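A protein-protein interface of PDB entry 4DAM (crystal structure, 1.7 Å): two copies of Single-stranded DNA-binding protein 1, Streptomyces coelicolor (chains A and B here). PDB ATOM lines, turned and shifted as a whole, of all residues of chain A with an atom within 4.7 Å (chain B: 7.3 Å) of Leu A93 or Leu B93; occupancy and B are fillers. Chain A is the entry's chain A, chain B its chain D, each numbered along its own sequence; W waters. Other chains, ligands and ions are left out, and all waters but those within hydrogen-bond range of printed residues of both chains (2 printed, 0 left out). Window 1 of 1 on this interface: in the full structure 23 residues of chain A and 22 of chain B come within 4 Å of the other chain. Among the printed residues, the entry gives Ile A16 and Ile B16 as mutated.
Water W1 bridges NZ of Lys A94 (3.0 Å) and O of His B61 (3.0 Å).
Water W2 lies within hydrogen-bond range of the backbone NH (N) of His B61 (3.0 Å) and the side-chain amino group (NZ) of Lys A94 (3.1 Å).
Printed residues of chain A that touch a printed residue of chain B: Ile A16, Ile A18, Asn A63, Leu A93, Lys A94, Val A95 and Ala A108.
Hydrophobic or aromatic side chains of chain A within 4 Å of the printed part of chain B: Ile A16, Ile A18, Leu A93, Val A95 and Ala A108.
Along chain A the printed residues that touch a printed residue of chain B span positions 16 to 108.
Of the 18 printed residues of chain B, 9 touch a printed residue of chain A.
Along chain B the printed residues that touch a printed residue of chain A span positions 16 to 108.
Among the printed residues, 18 pairs touch across the chains.
Among the printed residues, no Asp or Glu carboxylate lies within 4 Å of a Lys or Arg side-chain nitrogen of the other chain.
Printed residues of chain B within 4 Å of Asn A63: Leu B93, Lys B94 and Val B95.
Of chain B, only Ile B18, Asn B63, Phe B65 and Leu B93 come within 4 Å of Leu A93.
Printed residues of chain A within 4 Å of Leu B93: Asn A63 (2.9 Å) and Leu A93 (3.9 Å).
Of the printed residues of chain A, Val B95 touches Asn A63 (2.8 Å) and Ala A108 (3.8 Å).
Arg B96 touches none of the printed residues of chain A.
Of the printed residues of chain A, Ala B108 touches Val A95.
Asp B109 touches none of the printed residues of chain A.
The nearest printed residue of chain A that does not touch Leu B93 is Ile A18 (4.002 Å).
Asn A63 touches Leu B93, and with the chains exchanged Leu A93 touches Asn B63.
Asn A63 touches Val B95, and with the chains exchanged Val A95 touches Asn B63.
Leu A93 touches Phe B65, but with the chains exchanged Phe A65 does not touch Leu B93 (4.05 Å).
Val A95 touches Ala B108, and with the chains exchanged Ala A108 touches Val B95.
11 positions are printed for both chains.
Ile A16 touches Ile B18 (CG2 to CD1, 3.5 Å).
Asn B63 touches Ile A16.
CD1 of Ile A16 touches CE1 of Phe B65, at 3.7 Å.
Ile B16 touches Ile A18 (CG2 to CG1, 3.6 Å).
CD2 of Leu A93 touches CZ of Phe B65, at 3.9 Å.
Leu B93 touches Leu A93.
Lys A94 touches His B61 (CD to CD2, 3.9 Å).
Lys A94 touches Asn B63 (CA to ND2, 3.5 Å).
Val A95 touches Ala B108 (CG1 to CB, 3.8 Å).
CG2 of Val B95 touches CB of Ala A108 (3.8 Å).
The side-chain amide nitrogen (ND2) of Asn A63 lies close to the backbone NH (N) of Val B95 (2.8 Å).
ND2 of Asn B63 lies close to N of Val A95 (2.8 Å).
O of Leu A93 lies close to OD1 of Asn B63 (2.9 Å).
The backbone carbonyl oxygen of Val A95 is in hydrogen-bond range of a ring nitrogen (NE2) of His B61, at 2.9 Å.
The side-chain amide oxygen (OD1) of Asn A63 lies close to the backbone carbonyl oxygen (O) of Leu B93, 2.9 Å away.
The backbone carbonyl oxygen of Gly A91 is in hydrogen-bond range of the backbone NH of Ile A18 (2.9 Å).
The side-chain amide nitrogen of Asn B63 sits at hydrogen-bond distance from a ring nitrogen (NE2) of His B61, at 3.0 Å.
The backbone carbonyl oxygen (O) of Lys A94 sits at hydrogen-bond distance from the backbone NH (N) of Asp A109 (2.8 Å).
O of Lys B94 sits at hydrogen-bond distance from N of Asp B109 (2.8 Å).
The backbone carbonyl oxygen (O) of Ile B16 sits at hydrogen-bond distance from the backbone NH (N) of Leu B93 (2.8 Å).
The side-chain carboxylate (OD2) of Asp B111 lies within salt-bridge range of the side-chain amino group (NZ) of Lys B94 (2.9 Å).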
ATOM      1  N   ILE A  16       8.676  -2.906  -6.664  1.00  0.00           N
ATOM      2  CA  ILE A  16       8.497  -1.563  -6.172  1.00  0.00           C
ATOM      3  C   ILE A  16       9.803  -0.809  -6.412  1.00  0.00           C
ATOM      4  O   ILE A  16      10.803  -1.123  -5.799  1.00  0.00           O
ATOM      5  CB  ILE A  16       8.146  -1.600  -4.672  1.00  0.00           C
ATOM      6  CG1 ILE A  16       6.967  -2.568  -4.457  1.00  0.00           C
ATOM      7  CG2 ILE A  16       7.801  -0.194  -4.189  1.00  0.00           C
ATOM      8  CD1 ILE A  16       6.866  -3.269  -3.105  1.00  0.00           C
ATOM      9  N   ILE A  18      12.165   2.561  -6.288  1.00  0.00           N
ATOM     10  CA  ILE A  18      12.355   3.704  -5.417  1.00  0.00           C
ATOM     11  C   ILE A  18      13.514   4.527  -5.947  1.00  0.00           C
ATOM     12  O   ILE A  18      14.456   3.980  -6.525  1.00  0.00           O
ATOM     13  CB  ILE A  18      12.649   3.212  -3.978  1.00  0.00           C
ATOM     14  CG1 ILE A  18      12.885   4.317  -2.974  1.00  0.00           C
ATOM     15  CG2 ILE A  18      13.893   2.364  -3.925  1.00  0.00           C
ATOM     16  CD1 ILE A  18      13.115   3.703  -1.597  1.00  0.00           C
ATOM     17  N   ASN A  63      15.284   7.948   6.920  1.00  0.00           N
ATOM     18  CA  ASN A  63      15.179   6.584   6.432  1.00  0.00           C
ATOM     19  C   ASN A  63      16.589   6.038   6.201  1.00  0.00           C
ATOM     20  O   ASN A  63      17.386   6.642   5.458  1.00  0.00           O
ATOM     21  CB  ASN A  63      14.435   6.505   5.086  1.00  0.00           C
ATOM     22  CG  ASN A  63      12.907   6.619   5.193  1.00  0.00           C
ATOM     23  OD1 ASN A  63      12.209   6.956   4.204  1.00  0.00           O
ATOM     24  ND2 ASN A  63      12.379   6.333   6.349  1.00  0.00           N
ATOM     25  N   PHE A  65      18.617   2.783   4.506  1.00  0.00           N
ATOM     26  CA  PHE A  65      18.552   1.663   3.585  1.00  0.00           C
ATOM     27  C   PHE A  65      19.905   1.004   3.461  1.00  0.00           C
ATOM     28  O   PHE A  65      20.944   1.660   3.545  1.00  0.00           O
ATOM     29  CB  PHE A  65      18.156   2.114   2.187  1.00  0.00           C
ATOM     30  CG  PHE A  65      16.854   2.841   2.103  1.00  0.00           C
ATOM     31  CD1 PHE A  65      16.800   4.223   2.188  1.00  0.00           C
ATOM     32  CD2 PHE A  65      15.677   2.136   1.909  1.00  0.00           C
ATOM     33  CE1 PHE A  65      15.605   4.894   2.099  1.00  0.00           C
ATOM     34  CE2 PHE A  65      14.478   2.801   1.826  1.00  0.00           C
ATOM     35  CZ  PHE A  65      14.435   4.187   1.928  1.00  0.00           C
ATOM     36  N   GLY A  91      16.496   2.056  -7.554  1.00  0.00           N
ATOM     37  CA  GLY A  91      16.518   0.610  -7.581  1.00  0.00           C
ATOM     38  C   GLY A  91      15.271   0.002  -7.000  1.00  0.00           C
ATOM     39  O   GLY A  91      14.293   0.695  -6.758  1.00  0.00           O
ATOM     40  N   ARG A  92      15.314  -1.306  -6.795  1.00  0.00           N
ATOM     41  CA  ARG A  92      14.147  -2.039  -6.325  1.00  0.00           C
ATOM     42  C   ARG A  92      14.156  -2.149  -4.812  1.00  0.00           C
ATOM     43  O   ARG A  92      15.159  -2.567  -4.213  1.00  0.00           O
ATOM     44  CB  ARG A  92      14.147  -3.437  -6.942  1.00  0.00           C
ATOM     45  CG  ARG A  92      13.952  -3.383  -8.438  1.00  0.00           C
ATOM     46  CD  ARG A  92      13.838  -4.706  -9.127  1.00  0.00           C
ATOM     47  NE  ARG A  92      15.088  -5.105  -9.758  1.00  0.00           N
ATOM     48  CZ  ARG A  92      15.526  -4.652 -10.941  1.00  0.00           C
ATOM     49  NH1 ARG A  92      14.830  -3.775 -11.668  1.00  0.00           N
ATOM     50  NH2 ARG A  92      16.678  -5.092 -11.401  1.00  0.00           N
ATOM     51  N   LEU A  93      13.041  -1.799  -4.198  1.00  0.00           N
ATOM     52  CA  LEU A  93      12.907  -1.842  -2.744  1.00  0.00           C
ATOM     53  C   LEU A  93      12.561  -3.246  -2.273  1.00  0.00           C
ATOM     54  O   LEU A  93      11.619  -3.855  -2.790  1.00  0.00           O
ATOM     55  CB  LEU A  93      11.804  -0.884  -2.301  1.00  0.00           C
ATOM     56  CG  LEU A  93      11.459  -0.798  -0.805  1.00  0.00           C
ATOM     57  CD1 LEU A  93      12.618  -0.223   0.003  1.00  0.00           C
ATOM     58  CD2 LEU A  93      10.171  -0.024  -0.547  1.00  0.00           C
ATOM     59  N   LYS A  94      13.311  -3.730  -1.286  1.00  0.00           N
ATOM     60  CA  LYS A  94      13.014  -4.997  -0.619  1.00  0.00           C
ATOM     61  C   LYS A  94      12.931  -4.784   0.886  1.00  0.00           C
ATOM     62  O   LYS A  94      13.926  -4.446   1.519  1.00  0.00           O
ATOM     63  CB  LYS A  94      14.058  -6.049  -0.988  1.00  0.00           C
ATOM     64  CG  LYS A  94      14.246  -6.279  -2.494  1.00  0.00           C
ATOM     65  CD  LYS A  94      13.069  -7.005  -3.103  1.00  0.00           C
ATOM     66  CE  LYS A  94      12.971  -6.957  -4.635  1.00  0.00           C
ATOM     67  NZ  LYS A  94      11.842  -7.820  -5.122  1.00  0.00           N
ATOM     68  N   VAL A  95      11.727  -4.975   1.439  1.00  0.00           N
ATOM     69  CA  VAL A  95      11.467  -4.844   2.878  1.00  0.00           C
ATOM     70  C   VAL A  95      11.671  -6.221   3.470  1.00  0.00           C
ATOM     71  O   VAL A  95      11.063  -7.184   3.020  1.00  0.00           O
ATOM     72  CB  VAL A  95      10.008  -4.394   3.191  1.00  0.00           C
ATOM     73  CG1 VAL A  95       9.702  -4.404   4.704  1.00  0.00           C
ATOM     74  CG2 VAL A  95       9.726  -3.043   2.548  1.00  0.00           C
ATOM     75  N   ALA A 108      14.991  -2.089   5.392  1.00  0.00           N
ATOM     76  CA  ALA A 108      14.779  -1.830   3.973  1.00  0.00           C
ATOM     77  C   ALA A 108      16.086  -1.903   3.163  1.00  0.00           C
ATOM     78  O   ALA A 108      17.092  -1.241   3.484  1.00  0.00           O
ATOM     79  CB  ALA A 108      14.118  -0.478   3.839  1.00  0.00           C
ATOM     80  N   ASP A 109      16.065  -2.707   2.111  1.00  0.00           N
ATOM     81  CA  ASP A 109      17.176  -2.872   1.152  1.00  0.00           C
ATOM     82  C   ASP A 109      16.774  -2.191  -0.164  1.00  0.00           C
ATOM     83  O   ASP A 109      15.590  -2.175  -0.533  1.00  0.00           O
ATOM     84  CB  ASP A 109      17.442  -4.329   0.806  1.00  0.00           C
ATOM     85  CG  ASP A 109      18.142  -5.127   1.895  1.00  0.00           C
ATOM     86  OD1 ASP A 109      18.570  -4.602   2.913  1.00  0.00           O
ATOM     87  OD2 ASP A 109      18.288  -6.347   1.721  1.00  0.00           O
ATOM     88  N   GLU B  15      11.398  13.668   0.760  1.00  0.00           N
ATOM     89  CA  GLU B  15      10.541  12.567   1.115  1.00  0.00           C
ATOM     90  C   GLU B  15      10.744  11.497   0.045  1.00  0.00           C
ATOM     91  O   GLU B  15      11.069  11.795  -1.104  1.00  0.00           O
ATOM     92  CB  GLU B  15       9.093  13.040   1.162  1.00  0.00           C
ATOM     93  CG  GLU B  15       8.828  14.075   2.239  1.00  0.00           C
ATOM     94  CD  GLU B  15       8.473  13.461   3.572  1.00  0.00           C
ATOM     95  OE1 GLU B  15       8.739  12.252   3.787  1.00  0.00           O
ATOM     96  OE2 GLU B  15       7.898  14.193   4.402  1.00  0.00           O
ATOM     97  N   ILE B  16      10.579  10.239   0.440  1.00  0.00           N
ATOM     98  CA  ILE B  16      10.636   9.132  -0.505  1.00  0.00           C
ATOM     99  C   ILE B  16       9.205   8.726  -0.800  1.00  0.00           C
ATOM    100  O   ILE B  16       8.515   8.222   0.074  1.00  0.00           O
ATOM    101  CB  ILE B  16      11.342   7.872   0.034  1.00  0.00           C
ATOM    102  CG1 ILE B  16      12.823   8.092   0.283  1.00  0.00           C
ATOM    103  CG2 ILE B  16      11.161   6.713  -0.932  1.00  0.00           C
ATOM    104  CD1 ILE B  16      13.571   8.489  -0.949  1.00  0.00           C
ATOM    105  N   MET B  17       8.756   8.974  -2.019  1.00  0.00           N
ATOM    106  CA  MET B  17       7.408   8.580  -2.437  1.00  0.00           C
ATOM    107  C   MET B  17       7.461   7.135  -2.892  1.00  0.00           C
ATOM    108  O   MET B  17       8.501   6.626  -3.347  1.00  0.00           O
ATOM    109  CB  MET B  17       6.910   9.468  -3.594  1.00  0.00           C
ATOM    110  CG  MET B  17       6.660  10.925  -3.244  1.00  0.00           C
ATOM    111  SD  MET B  17       5.773  11.190  -1.707  1.00  0.00           S
ATOM    112  CE  MET B  17       4.135  10.459  -1.981  1.00  0.00           C
ATOM    113  N   ILE B  18       6.350   6.449  -2.725  1.00  0.00           N
ATOM    114  CA  ILE B  18       6.222   5.089  -3.212  1.00  0.00           C
ATOM    115  C   ILE B  18       4.818   4.903  -3.748  1.00  0.00           C
ATOM    116  O   ILE B  18       3.863   5.507  -3.250  1.00  0.00           O
ATOM    117  CB  ILE B  18       6.499   4.084  -2.079  1.00  0.00           C
ATOM    118  CG1 ILE B  18       6.399   2.636  -2.516  1.00  0.00           C
ATOM    119  CG2 ILE B  18       5.540   4.273  -0.926  1.00  0.00           C
ATOM    120  CD1 ILE B  18       6.797   1.719  -1.374  1.00  0.00           C
ATOM    121  N   HIS B  61       9.518 -12.305  -3.956  1.00  0.00           N
ATOM    122  CA  HIS B  61       9.495 -11.738  -2.620  1.00  0.00           C
ATOM    123  C   HIS B  61       8.234 -10.927  -2.385  1.00  0.00           C
ATOM    124  O   HIS B  61       7.779 -10.201  -3.278  1.00  0.00           O
ATOM    125  CB  HIS B  61      10.718 -10.841  -2.447  1.00  0.00           C
ATOM    126  CG  HIS B  61      10.797 -10.136  -1.119  1.00  0.00           C
ATOM    127  ND1 HIS B  61      11.135 -10.762   0.027  1.00  0.00           N
ATOM    128  CD2 HIS B  61      10.568  -8.804  -0.791  1.00  0.00           C
ATOM    129  CE1 HIS B  61      11.097  -9.880   1.054  1.00  0.00           C
ATOM    130  NE2 HIS B  61      10.774  -8.676   0.553  1.00  0.00           N
ATOM    131  N   ASN B  63       6.847  -7.860  -0.214  1.00  0.00           N
ATOM    132  CA  ASN B  63       7.068  -6.715   0.644  1.00  0.00           C
ATOM    133  C   ASN B  63       5.805  -6.485   1.459  1.00  0.00           C
ATOM    134  O   ASN B  63       4.710  -6.368   0.868  1.00  0.00           O
ATOM    135  CB  ASN B  63       7.320  -5.455  -0.178  1.00  0.00           C
ATOM    136  CG  ASN B  63       8.746  -5.320  -0.704  1.00  0.00           C
ATOM    137  OD1 ASN B  63       9.015  -4.533  -1.680  1.00  0.00           O
ATOM    138  ND2 ASN B  63       9.662  -6.009  -0.074  1.00  0.00           N
ATOM    139  N   PHE B  65       3.997  -3.835   4.097  1.00  0.00           N
ATOM    140  CA  PHE B  65       3.980  -2.474   4.587  1.00  0.00           C
ATOM    141  C   PHE B  65       2.818  -2.294   5.544  1.00  0.00           C
ATOM    142  O   PHE B  65       1.767  -2.916   5.369  1.00  0.00           O
ATOM    143  CB  PHE B  65       3.770  -1.480   3.445  1.00  0.00           C
ATOM    144  CG  PHE B  65       4.795  -1.535   2.376  1.00  0.00           C
ATOM    145  CD1 PHE B  65       4.624  -2.317   1.246  1.00  0.00           C
ATOM    146  CD2 PHE B  65       5.950  -0.773   2.480  1.00  0.00           C
ATOM    147  CE1 PHE B  65       5.564  -2.350   0.242  1.00  0.00           C
ATOM    148  CE2 PHE B  65       6.884  -0.801   1.476  1.00  0.00           C
ATOM    149  CZ  PHE B  65       6.721  -1.607   0.373  1.00  0.00           C
ATOM    150  N   GLY B  91       2.030   6.981  -1.419  1.00  0.00           N
ATOM    151  CA  GLY B  91       2.301   7.780  -0.234  1.00  0.00           C
ATOM    152  C   GLY B  91       3.773   7.869   0.078  1.00  0.00           C
ATOM    153  O   GLY B  91       4.607   7.499  -0.724  1.00  0.00           O
ATOM    154  N   ARG B  92       4.069   8.329   1.277  1.00  0.00           N
ATOM    155  CA  ARG B  92       5.435   8.533   1.697  1.00  0.00           C
ATOM    156  C   ARG B  92       5.939   7.326   2.483  1.00  0.00           C
ATOM    157  O   ARG B  92       5.281   6.879   3.416  1.00  0.00           O
ATOM    158  CB  ARG B  92       5.489   9.798   2.572  1.00  0.00           C
ATOM    159  CG  ARG B  92       5.149  11.063   1.804  1.00  0.00           C
ATOM    160  CD  ARG B  92       5.126  12.268   2.729  1.00  0.00           C
ATOM    161  NE  ARG B  92       4.014  12.163   3.660  1.00  0.00           N
ATOM    162  CZ  ARG B  92       2.766  12.577   3.421  1.00  0.00           C
ATOM    163  NH1 ARG B  92       2.447  13.197   2.283  1.00  0.00           N
ATOM    164  NH2 ARG B  92       1.833  12.390   4.339  1.00  0.00           N
ATOM    165  N   LEU B  93       7.111   6.827   2.099  1.00  0.00           N
ATOM    166  CA  LEU B  93       7.729   5.681   2.765  1.00  0.00           C
ATOM    167  C   LEU B  93       8.466   6.116   4.019  1.00  0.00           C
ATOM    168  O   LEU B  93       9.270   7.046   3.972  1.00  0.00           O
ATOM    169  CB  LEU B  93       8.693   4.994   1.812  1.00  0.00           C
ATOM    170  CG  LEU B  93       9.433   3.781   2.364  1.00  0.00           C
ATOM    171  CD1 LEU B  93       8.438   2.684   2.722  1.00  0.00           C
ATOM    172  CD2 LEU B  93      10.483   3.293   1.390  1.00  0.00           C
ATOM    173  N   LYS B  94       8.171   5.455   5.132  1.00  0.00           N
ATOM    174  CA  LYS B  94       8.872   5.686   6.391  1.00  0.00           C
ATOM    175  C   LYS B  94       9.359   4.354   6.945  1.00  0.00           C
ATOM    176  O   LYS B  94       8.561   3.484   7.290  1.00  0.00           O
ATOM    177  CB  LYS B  94       7.967   6.368   7.418  1.00  0.00           C
ATOM    178  CG  LYS B  94       7.366   7.652   6.945  1.00  0.00           C
ATOM    179  CD  LYS B  94       8.349   8.752   6.885  1.00  0.00           C
ATOM    180  CE  LYS B  94       7.542   9.847   6.204  1.00  0.00           C
ATOM    181  NZ  LYS B  94       6.419  10.401   7.013  1.00  0.00           N
ATOM    182  N   VAL B  95      10.669   4.184   6.982  1.00  0.00           N
ATOM    183  CA  VAL B  95      11.310   3.009   7.528  1.00  0.00           C
ATOM    184  C   VAL B  95      11.632   3.356   8.980  1.00  0.00           C
ATOM    185  O   VAL B  95      12.455   4.232   9.254  1.00  0.00           O
ATOM    186  CB  VAL B  95      12.561   2.624   6.699  1.00  0.00           C
ATOM    187  CG1 VAL B  95      13.207   1.363   7.262  1.00  0.00           C
ATOM    188  CG2 VAL B  95      12.210   2.485   5.207  1.00  0.00           C
ATOM    189  N   ARG B  96      10.932   2.708   9.915  1.00  0.00           N
ATOM    190  CA  ARG B  96      10.890   3.156  11.332  1.00  0.00           C
ATOM    191  C   ARG B  96      11.579   2.189  12.264  1.00  0.00           C
ATOM    192  O   ARG B  96      11.526   0.975  12.047  1.00  0.00           O
ATOM    193  CB  ARG B  96       9.447   3.305  11.812  1.00  0.00           C
ATOM    194  CG  ARG B  96       8.707   4.346  11.081  1.00  0.00           C
ATOM    195  CD  ARG B  96       7.555   4.835  11.898  1.00  0.00           C
ATOM    196  NE  ARG B  96       6.763   5.842  11.216  1.00  0.00           N
ATOM    197  CZ  ARG B  96       7.003   7.156  11.203  1.00  0.00           C
ATOM    198  NH1 ARG B  96       8.063   7.696  11.816  1.00  0.00           N
ATOM    199  NH2 ARG B  96       6.152   7.938  10.547  1.00  0.00           N
ATOM    200  N   SER B 107       9.130  -0.928  11.668  1.00  0.00           N
ATOM    201  CA  SER B 107       8.096  -0.984  10.619  1.00  0.00           C
ATOM    202  C   SER B 107       8.587  -0.422   9.303  1.00  0.00           C
ATOM    203  O   SER B 107       9.549   0.330   9.304  1.00  0.00           O
ATOM    204  CB  SER B 107       6.845  -0.224  11.061  1.00  0.00           C
ATOM    205  OG  SER B 107       5.684  -0.842  10.509  1.00  0.00           O
ATOM    206  N   ALA B 108       7.999  -0.877   8.188  1.00  0.00           N
ATOM    207  CA  ALA B 108       8.068  -0.134   6.927  1.00  0.00           C
ATOM    208  C   ALA B 108       6.677   0.357   6.683  1.00  0.00           C
ATOM    209  O   ALA B 108       5.769  -0.447   6.436  1.00  0.00           O
ATOM    210  CB  ALA B 108       8.538  -0.971   5.759  1.00  0.00           C
ATOM    211  N   ASP B 109       6.519   1.652   6.817  1.00  0.00           N
ATOM    212  CA  ASP B 109       5.226   2.300   6.826  1.00  0.00           C
ATOM    213  C   ASP B 109       5.055   3.053   5.505  1.00  0.00           C
ATOM    214  O   ASP B 109       6.009   3.565   4.937  1.00  0.00           O
ATOM    215  CB  ASP B 109       5.126   3.319   7.944  1.00  0.00           C
ATOM    216  CG  ASP B 109       4.975   2.709   9.337  1.00  0.00           C
ATOM    217  OD1 ASP B 109       4.842   1.468   9.493  1.00  0.00           O
ATOM    218  OD2 ASP B 109       4.981   3.531  10.305  1.00  0.00           O
ATOM    219  N   ILE B 110       3.817   3.142   5.046  1.00  0.00           N
ATOM    220  CA  ILE B 110       3.462   4.075   4.010  1.00  0.00           C
ATOM    221  C   ILE B 110       2.425   5.017   4.603  1.00  0.00           C
ATOM    222  O   ILE B 110       1.352   4.603   5.031  1.00  0.00           O
ATOM    223  CB  ILE B 110       2.880   3.410   2.733  1.00  0.00           C
ATOM    224  CG1 ILE B 110       3.877   2.427   2.126  1.00  0.00           C
ATOM    225  CG2 ILE B 110       2.462   4.484   1.727  1.00  0.00           C
ATOM    226  CD1 ILE B 110       3.338   1.573   1.011  1.00  0.00           C
ATOM    227  N   ASP B 111       2.752   6.305   4.624  1.00  0.00           N
ATOM    228  CA  ASP B 111       1.803   7.341   4.998  1.00  0.00           C
ATOM    229  C   ASP B 111       1.052   7.721   3.722  1.00  0.00           C
ATOM    230  O   ASP B 111       1.573   8.419   2.836  1.00  0.00           O
ATOM    231  CB  ASP B 111       2.520   8.534   5.608  1.00  0.00           C
ATOM    232  CG  ASP B 111       3.061   8.244   6.993  1.00  0.00           C
ATOM    233  OD1 ASP B 111       2.666   7.221   7.616  1.00  0.00           O
ATOM    234  OD2 ASP B 111       3.878   9.058   7.477  1.00  0.00           O
HETATM  235  O   HOH W   1       9.236  -7.640  -3.715  1.00  0.00           O
HETATM  236  O   HOH W   2      11.385 -10.778  -5.765  1.00  0.00           O
